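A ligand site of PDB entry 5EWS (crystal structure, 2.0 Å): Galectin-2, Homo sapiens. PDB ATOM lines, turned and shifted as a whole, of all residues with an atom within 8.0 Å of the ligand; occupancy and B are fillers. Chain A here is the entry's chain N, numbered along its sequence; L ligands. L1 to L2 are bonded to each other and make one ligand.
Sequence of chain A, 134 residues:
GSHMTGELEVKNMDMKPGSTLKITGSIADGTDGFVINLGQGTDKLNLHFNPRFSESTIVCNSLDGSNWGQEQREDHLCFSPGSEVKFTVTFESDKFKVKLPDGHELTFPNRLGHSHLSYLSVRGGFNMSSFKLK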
ATOM      1  N   PHE A  34      -6.000  24.753  -6.450  1.00  0.00           N
ATOM      2  CA  PHE A  34      -4.883  25.499  -5.879  1.00  0.00           C
ATOM      3  C   PHE A  34      -5.036  25.509  -4.369  1.00  0.00           C
ATOM      4  O   PHE A  34      -6.020  25.025  -3.813  1.00  0.00           O
ATOM      5  CB  PHE A  34      -4.817  26.924  -6.451  1.00  0.00           C
ATOM      6  CG  PHE A  34      -5.972  27.802  -6.067  1.00  0.00           C
ATOM      7  CD1 PHE A  34      -7.108  27.848  -6.858  1.00  0.00           C
ATOM      8  CD2 PHE A  34      -5.927  28.583  -4.924  1.00  0.00           C
ATOM      9  CE1 PHE A  34      -8.178  28.653  -6.514  1.00  0.00           C
ATOM     10  CE2 PHE A  34      -6.987  29.385  -4.571  1.00  0.00           C
ATOM     11  CZ  PHE A  34      -8.118  29.422  -5.371  1.00  0.00           C
ATOM     12  N   VAL A  35      -4.025  26.067  -3.704  1.00  0.00           N
ATOM     13  CA  VAL A  35      -3.894  25.985  -2.258  1.00  0.00           C
ATOM     14  C   VAL A  35      -3.510  27.353  -1.703  1.00  0.00           C
ATOM     15  O   VAL A  35      -2.626  28.026  -2.246  1.00  0.00           O
ATOM     16  CB  VAL A  35      -2.849  24.927  -1.840  1.00  0.00           C
ATOM     17  CG1 VAL A  35      -2.538  25.048  -0.370  1.00  0.00           C
ATOM     18  CG2 VAL A  35      -3.367  23.529  -2.153  1.00  0.00           C
ATOM     19  N   ASN A  37      -2.113  28.417   1.926  1.00  0.00           N
ATOM     20  CA  ASN A  37      -1.640  27.928   3.219  1.00  0.00           C
ATOM     21  C   ASN A  37      -1.315  29.128   4.099  1.00  0.00           C
ATOM     22  O   ASN A  37      -0.661  30.076   3.661  1.00  0.00           O
ATOM     23  CB  ASN A  37      -0.401  27.038   3.068  1.00  0.00           C
ATOM     24  CG  ASN A  37      -0.730  25.698   2.446  1.00  0.00           C
ATOM     25  OD1 ASN A  37      -1.734  25.073   2.784  1.00  0.00           O
ATOM     26  ND2 ASN A  37       0.142  25.239   1.552  1.00  0.00           N
ATOM     27  N   LEU A  45       0.544  24.527   9.708  1.00  0.00           N
ATOM     28  CA  LEU A  45      -0.447  25.247   8.926  1.00  0.00           C
ATOM     29  C   LEU A  45      -1.764  25.276   9.706  1.00  0.00           C
ATOM     30  O   LEU A  45      -2.439  24.255   9.836  1.00  0.00           O
ATOM     31  CB  LEU A  45      -0.656  24.614   7.555  1.00  0.00           C
ATOM     32  CG  LEU A  45       0.537  24.468   6.609  1.00  0.00           C
ATOM     33  CD1 LEU A  45       0.127  23.749   5.331  1.00  0.00           C
ATOM     34  CD2 LEU A  45       1.100  25.847   6.284  1.00  0.00           C
ATOM     35  N   HIS A  48      -5.260  25.290   5.904  1.00  0.00           N
ATOM     36  CA  HIS A  48      -4.940  24.802   4.574  1.00  0.00           C
ATOM     37  C   HIS A  48      -6.206  24.895   3.735  1.00  0.00           C
ATOM     38  O   HIS A  48      -7.143  24.126   3.932  1.00  0.00           O
ATOM     39  CB  HIS A  48      -4.416  23.376   4.612  1.00  0.00           C
ATOM     40  CG  HIS A  48      -4.312  22.734   3.261  1.00  0.00           C
ATOM     41  ND1 HIS A  48      -3.249  22.959   2.415  1.00  0.00           N
ATOM     42  CD2 HIS A  48      -5.136  21.890   2.604  1.00  0.00           C
ATOM     43  CE1 HIS A  48      -3.427  22.270   1.296  1.00  0.00           C
ATOM     44  NE2 HIS A  48      -4.562  21.618   1.383  1.00  0.00           N
ATOM     45  N   PHE A  49      -6.224  25.841   2.796  1.00  0.00           N
ATOM     46  CA  PHE A  49      -7.407  26.197   2.028  1.00  0.00           C
ATOM     47  C   PHE A  49      -7.188  25.740   0.593  1.00  0.00           C
ATOM     48  O   PHE A  49      -6.354  26.302  -0.115  1.00  0.00           O
ATOM     49  CB  PHE A  49      -7.633  27.709   2.101  1.00  0.00           C
ATOM     50  CG  PHE A  49      -8.763  28.209   1.258  1.00  0.00           C
ATOM     51  CD1 PHE A  49     -10.082  28.032   1.662  1.00  0.00           C
ATOM     52  CD2 PHE A  49      -8.519  28.862   0.059  1.00  0.00           C
ATOM     53  CE1 PHE A  49     -11.120  28.506   0.893  1.00  0.00           C
ATOM     54  CE2 PHE A  49      -9.560  29.332  -0.720  1.00  0.00           C
ATOM     55  CZ  PHE A  49     -10.866  29.156  -0.297  1.00  0.00           C
ATOM     56  N   ASN A  50      -7.947  24.726   0.154  1.00  0.00           N
ATOM     57  CA  ASN A  50      -7.629  24.000  -1.081  1.00  0.00           C
ATOM     58  C   ASN A  50      -8.890  23.783  -1.911  1.00  0.00           C
ATOM     59  O   ASN A  50      -9.516  22.723  -1.845  1.00  0.00           O
ATOM     60  CB  ASN A  50      -6.946  22.665  -0.767  1.00  0.00           C
ATOM     61  CG  ASN A  50      -6.630  21.845  -2.013  1.00  0.00           C
ATOM     62  OD1 ASN A  50      -6.469  20.632  -1.933  1.00  0.00           O
ATOM     63  ND2 ASN A  50      -6.533  22.518  -3.158  1.00  0.00           N
ATOM     64  N   PRO A  51      -9.288  24.779  -2.703  1.00  0.00           N
ATOM     65  CA  PRO A  51     -10.337  24.548  -3.703  1.00  0.00           C
ATOM     66  C   PRO A  51      -9.838  23.584  -4.781  1.00  0.00           C
ATOM     67  O   PRO A  51      -8.756  23.758  -5.331  1.00  0.00           O
ATOM     68  CB  PRO A  51     -10.593  25.942  -4.280  1.00  0.00           C
ATOM     69  CG  PRO A  51     -10.086  26.890  -3.239  1.00  0.00           C
ATOM     70  CD  PRO A  51      -8.901  26.196  -2.614  1.00  0.00           C
ATOM     71  N   ARG A  52     -10.654  22.575  -5.077  1.00  0.00           N
ATOM     72  CA  ARG A  52     -10.333  21.566  -6.082  1.00  0.00           C
ATOM     73  C   ARG A  52     -11.454  21.569  -7.124  1.00  0.00           C
ATOM     74  O   ARG A  52     -12.534  21.019  -6.879  1.00  0.00           O
ATOM     75  CB  ARG A  52     -10.162  20.188  -5.435  1.00  0.00           C
ATOM     76  CG  ARG A  52      -9.083  20.124  -4.361  1.00  0.00           C
ATOM     77  CD  ARG A  52      -9.063  18.775  -3.652  1.00  0.00           C
ATOM     78  NE  ARG A  52      -8.173  18.776  -2.486  1.00  0.00           N
ATOM     79  CZ  ARG A  52      -8.109  17.788  -1.599  1.00  0.00           C
ATOM     80  NH1 ARG A  52      -8.893  16.720  -1.719  1.00  0.00           N
ATOM     81  NH2 ARG A  52      -7.270  17.874  -0.570  1.00  0.00           N
ATOM     82  N   GLU A  55     -12.903  18.238  -8.196  1.00  0.00           N
ATOM     83  CA  GLU A  55     -13.734  17.592  -7.197  1.00  0.00           C
ATOM     84  C   GLU A  55     -14.922  18.435  -6.770  1.00  0.00           C
ATOM     85  O   GLU A  55     -15.697  18.008  -5.917  1.00  0.00           O
ATOM     86  CB  GLU A  55     -12.879  17.225  -5.980  1.00  0.00           C
ATOM     87  CG  GLU A  55     -11.703  16.314  -6.314  1.00  0.00           C
ATOM     88  CD  GLU A  55     -10.884  15.937  -5.096  1.00  0.00           C
ATOM     89  OE1 GLU A  55     -11.415  15.981  -3.969  1.00  0.00           O
ATOM     90  OE2 GLU A  55      -9.693  15.594  -5.273  1.00  0.00           O
ATOM     91  N   VAL A  59     -11.580  21.836   0.159  1.00  0.00           N
ATOM     92  CA  VAL A  59     -11.059  21.153   1.323  1.00  0.00           C
ATOM     93  C   VAL A  59     -10.307  22.154   2.183  1.00  0.00           C
ATOM     94  O   VAL A  59      -9.421  22.864   1.704  1.00  0.00           O
ATOM     95  CB  VAL A  59     -10.154  19.978   0.923  1.00  0.00           C
ATOM     96  CG1 VAL A  59      -9.776  19.166   2.147  1.00  0.00           C
ATOM     97  CG2 VAL A  59     -10.866  19.102  -0.090  1.00  0.00           C
ATOM     98  N   CYS A  60     -10.672  22.213   3.469  1.00  0.00           N
ATOM     99  CA  CYS A  60      -9.925  22.946   4.469  1.00  0.00           C
ATOM    100  C   CYS A  60      -9.383  21.961   5.482  1.00  0.00           C
ATOM    101  O   CYS A  60     -10.060  20.997   5.855  1.00  0.00           O
ATOM    102  CB  CYS A  60     -10.793  24.000   5.175  1.00  0.00           C
ATOM    103  SG  CYS A  60     -11.540  25.232   4.084  1.00  0.00           S
ATOM    104  N   ASN A  61      -8.142  22.176   5.925  1.00  0.00           N
ATOM    105  CA  ASN A  61      -7.543  21.298   6.907  1.00  0.00           C
ATOM    106  C   ASN A  61      -6.460  22.062   7.656  1.00  0.00           C
ATOM    107  O   ASN A  61      -6.162  23.221   7.346  1.00  0.00           O
ATOM    108  CB  ASN A  61      -6.976  20.029   6.246  1.00  0.00           C
ATOM    109  CG  ASN A  61      -6.941  18.847   7.187  1.00  0.00           C
ATOM    110  OD1 ASN A  61      -7.235  18.980   8.384  1.00  0.00           O
ATOM    111  ND2 ASN A  61      -6.584  17.681   6.675  1.00  0.00           N
ATOM    112  N   SER A  62      -5.863  21.392   8.632  1.00  0.00           N
ATOM    113  CA  SER A  62      -4.745  21.926   9.398  1.00  0.00           C
ATOM    114  C   SER A  62      -3.580  20.957   9.327  1.00  0.00           C
ATOM    115  O   SER A  62      -3.752  19.756   9.085  1.00  0.00           O
ATOM    116  CB  SER A  62      -5.153  22.158  10.863  1.00  0.00           C
ATOM    117  OG  SER A  62      -5.809  21.032  11.396  1.00  0.00           O
ATOM    118  N   LEU A  63      -2.379  21.492   9.547  1.00  0.00           N
ATOM    119  CA  LEU A  63      -1.168  20.694   9.459  1.00  0.00           C
ATOM    120  C   LEU A  63      -0.289  21.001  10.673  1.00  0.00           C
ATOM    121  O   LEU A  63       0.099  22.156  10.875  1.00  0.00           O
ATOM    122  CB  LEU A  63      -0.398  20.984   8.164  1.00  0.00           C
ATOM    123  CG  LEU A  63       0.949  20.290   8.015  1.00  0.00           C
ATOM    124  CD1 LEU A  63       0.764  18.792   7.826  1.00  0.00           C
ATOM    125  CD2 LEU A  63       1.729  20.885   6.850  1.00  0.00           C
ATOM    126  N   TRP A  68      -1.483  15.621   9.295  1.00  0.00           N
ATOM    127  CA  TRP A  68      -2.660  16.366   8.869  1.00  0.00           C
ATOM    128  C   TRP A  68      -3.807  16.159   9.840  1.00  0.00           C
ATOM    129  O   TRP A  68      -3.974  15.091  10.433  1.00  0.00           O
ATOM    130  CB  TRP A  68      -3.106  15.946   7.463  1.00  0.00           C
ATOM    131  CG  TRP A  68      -2.254  16.474   6.347  1.00  0.00           C
ATOM    132  CD1 TRP A  68      -1.261  15.803   5.681  1.00  0.00           C
ATOM    133  CD2 TRP A  68      -2.339  17.771   5.749  1.00  0.00           C
ATOM    134  NE1 TRP A  68      -0.725  16.617   4.710  1.00  0.00           N
ATOM    135  CE2 TRP A  68      -1.363  17.828   4.733  1.00  0.00           C
ATOM    136  CE3 TRP A  68      -3.135  18.893   5.976  1.00  0.00           C
ATOM    137  CZ2 TRP A  68      -1.168  18.963   3.946  1.00  0.00           C
ATOM    138  CZ3 TRP A  68      -2.947  20.020   5.192  1.00  0.00           C
ATOM    139  CH2 TRP A  68      -1.967  20.037   4.190  1.00  0.00           C
ATOM    140  N   GLY A  69      -4.612  17.208  10.007  1.00  0.00           N
ATOM    141  CA  GLY A  69      -5.815  17.123  10.797  1.00  0.00           C
ATOM    142  C   GLY A  69      -6.921  16.422  10.042  1.00  0.00           C
ATOM    143  O   GLY A  69      -6.688  15.693   9.071  1.00  0.00           O
ATOM    144  N   GLN A  70      -8.145  16.656  10.485  1.00  0.00           N
ATOM    145  CA  GLN A  70      -9.320  16.080   9.836  1.00  0.00           C
ATOM    146  C   GLN A  70      -9.853  17.058   8.801  1.00  0.00           C
ATOM    147  O   GLN A  70     -10.142  18.213   9.125  1.00  0.00           O
ATOM    148  CB  GLN A  70     -10.392  15.736  10.868  1.00  0.00           C
ATOM    149  CG  GLN A  70     -11.767  15.496  10.273  1.00  0.00           C
ATOM    150  CD  GLN A  70     -12.688  14.744  11.202  1.00  0.00           C
ATOM    151  OE1 GLN A  70     -13.907  14.937  11.156  1.00  0.00           O
ATOM    152  NE2 GLN A  70     -12.120  13.881  12.034  1.00  0.00           N
ATOM    153  N   GLU A  71     -10.006  16.587   7.565  1.00  0.00           N
ATOM    154  CA  GLU A  71     -10.400  17.464   6.476  1.00  0.00           C
ATOM    155  C   GLU A  71     -11.843  17.930   6.643  1.00  0.00           C
ATOM    156  O   GLU A  71     -12.698  17.197   7.155  1.00  0.00           O
ATOM    157  CB  GLU A  71     -10.256  16.762   5.136  1.00  0.00           C
ATOM    158  CG  GLU A  71      -8.882  16.224   4.815  1.00  0.00           C
ATOM    159  CD  GLU A  71      -8.804  15.626   3.423  1.00  0.00           C
ATOM    160  OE1 GLU A  71      -7.692  15.531   2.862  1.00  0.00           O
ATOM    161  OE2 GLU A  71      -9.864  15.246   2.882  1.00  0.00           O
ATOM    162  N   GLN A  72     -12.100  19.148   6.194  1.00  0.00           N
ATOM    163  CA  GLN A  72     -13.422  19.738   6.133  1.00  0.00           C
ATOM    164  C   GLN A  72     -13.727  20.136   4.697  1.00  0.00           C
ATOM    165  O   GLN A  72     -13.066  21.025   4.148  1.00  0.00           O
ATOM    166  CB  GLN A  72     -13.518  20.949   7.053  1.00  0.00           C
ATOM    167  CG  GLN A  72     -14.813  21.716   6.956  1.00  0.00           C
ATOM    168  CD  GLN A  72     -14.936  22.772   8.024  1.00  0.00           C
ATOM    169  OE1 GLN A  72     -14.326  22.663   9.093  1.00  0.00           O
ATOM    170  NE2 GLN A  72     -15.658  23.853   7.722  1.00  0.00           N
ATOM    171  N   ARG A  73     -14.715  19.487   4.091  1.00  0.00           N
ATOM    172  CA  ARG A  73     -15.064  19.764   2.709  1.00  0.00           C
ATOM    173  C   ARG A  73     -16.290  20.657   2.658  1.00  0.00           C
ATOM    174  O   ARG A  73     -17.270  20.428   3.375  1.00  0.00           O
ATOM    175  CB  ARG A  73     -15.302  18.487   1.910  1.00  0.00           C
ATOM    176  CG  ARG A  73     -14.116  17.550   1.975  1.00  0.00           C
ATOM    177  CD  ARG A  73     -14.106  16.545   0.842  1.00  0.00           C
ATOM    178  NE  ARG A  73     -12.803  15.897   0.775  1.00  0.00           N
ATOM    179  CZ  ARG A  73     -12.267  15.380  -0.317  1.00  0.00           C
ATOM    180  NH1 ARG A  73     -12.915  15.439  -1.479  1.00  0.00           N
ATOM    181  NH2 ARG A  73     -11.060  14.827  -0.272  1.00  0.00           N
ATOM    182  N   ARG A 123      -0.015  27.692  -3.504  1.00  0.00           N
ATOM    183  CA  ARG A 123       0.372  26.557  -4.319  1.00  0.00           C
ATOM    184  C   ARG A 123      -0.597  26.422  -5.482  1.00  0.00           C
ATOM    185  O   ARG A 123      -1.680  27.012  -5.496  1.00  0.00           O
ATOM    186  CB  ARG A 123       0.405  25.260  -3.500  1.00  0.00           C
ATOM    187  CG  ARG A 123       1.229  25.359  -2.221  1.00  0.00           C
ATOM    188  CD  ARG A 123       2.698  25.081  -2.483  1.00  0.00           C
ATOM    189  NE  ARG A 123       3.519  25.322  -1.296  1.00  0.00           N
ATOM    190  CZ  ARG A 123       4.079  26.480  -0.998  1.00  0.00           C
ATOM    191  NH1 ARG A 123       3.912  27.523  -1.801  1.00  0.00           N
ATOM    192  NH2 ARG A 123       4.811  26.601   0.101  1.00  0.00           N
HETATM  193  C1  LIG L   1      -6.426  11.859   0.736  1.00  0.00           C
HETATM  194  C2  LIG L   1      -6.206  13.182   0.105  1.00  0.00           C
HETATM  195  C3  LIG L   1      -4.887  13.689   0.435  1.00  0.00           C
HETATM  196  C4  LIG L   1      -3.848  12.790  -0.140  1.00  0.00           C
HETATM  197  C5  LIG L   1      -2.443  13.173   0.266  1.00  0.00           C
HETATM  198  C6  LIG L   1      -5.415  10.826   0.215  1.00  0.00           C
HETATM  199  O1  LIG L   1      -5.508   9.743   0.947  1.00  0.00           O
HETATM  200  O2  LIG L   1      -7.752  11.375   0.432  1.00  0.00           O
HETATM  201  O3  LIG L   1      -7.239  14.153   0.512  1.00  0.00           O
HETATM  202  O4  LIG L   1      -4.827  15.161   0.033  1.00  0.00           O
HETATM  203  O5  LIG L   1      -4.006  11.406   0.333  1.00  0.00           O
HETATM  204  O6  LIG L   1      -2.193  12.627   1.539  1.00  0.00           O
HETATM  205  C1  LG2 L   2      -3.645  15.817   0.380  1.00  0.00           C
HETATM  206  C2  LG2 L   2      -3.318  16.889  -0.660  1.00  0.00           C
HETATM  207  C3  LG2 L   2      -3.210  18.300  -0.213  1.00  0.00           C
HETATM  208  C4  LG2 L   2      -3.985  18.662   0.996  1.00  0.00           C
HETATM  209  C5  LG2 L   2      -4.218  17.590   2.033  1.00  0.00           C
HETATM  210  C6  LG2 L   2      -5.655  17.490   2.430  1.00  0.00           C
HETATM  211  O1  LG2 L   2      -2.198  16.500  -1.502  1.00  0.00           O
HETATM  212  O2  LG2 L   2      -3.655  19.150  -1.302  1.00  0.00           O
HETATM  213  O3  LG2 L   2      -5.240  19.276   0.603  1.00  0.00           O
HETATM  214  O4  LG2 L   2      -3.610  16.256   1.777  1.00  0.00           O
HETATM  215  O5  LG2 L   2      -5.654  17.076   3.765  1.00  0.00           O
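A ring nitrogen (NE2) of His 48 sits at hydrogen-bond distance from an oxygen (O3) of LG2 L2 (2.6 Å). OD1 of Asn 50 is in hydrogen-bond range of O3 of LG2 L2 (3.1 Å). O5 of LG2 L2 sits at hydrogen-bond distance from OE1 of Glu 71 (2.7 Å). The side-chain amide nitrogen of Asn 61 is in hydrogen-bond range of an oxygen (O5) of LG2 L2, at 3.1 Å. The guanidinium group (NH2) of Arg 52 lies within hydrogen-bond range of an oxygen (O3) of LG2 L2 (2.7 Å).
The side-chain carboxylate (OE1) of Glu 55 lies within salt-bridge range of the guanidinium group (NH1) of Arg 73 (3.0 Å). The guanidinium group of Arg 52 lies within hydrogen-bond range of the side-chain amide oxygen of Asn 50. The backbone NH of Asn 50 is in hydrogen-bond range of the backbone carbonyl oxygen of Val 59, 2.8 Å away. The backbone NH (N) of His 48 sits at hydrogen-bond distance from the backbone carbonyl oxygen (O) of Asn 61, at 2.7 Å. NH2 of Arg 73 lies within salt-bridge range of OE2 of Glu 71 (3.4 Å). The side-chain amide nitrogen (ND2) of Asn 61 lies within hydrogen-bond range of the backbone carbonyl oxygen (O) of Gly 69 (3.1 Å). O of Gln 70 lies close to OD1 of Asn 61 (3.1 Å). The guanidinium group (NH1) of Arg 52 is in salt-bridge range of the side-chain carboxylate (OE1) of Glu 55 (3.5 Å).
Merely in contact with the ligand: Trp 68 (3.8 Å) and Arg 73 (3.96 Å). Within 4 Å of the ligand: His 48, Asn 50, Arg 52, Asn 61, Trp 68, Glu 71 and Arg 73.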
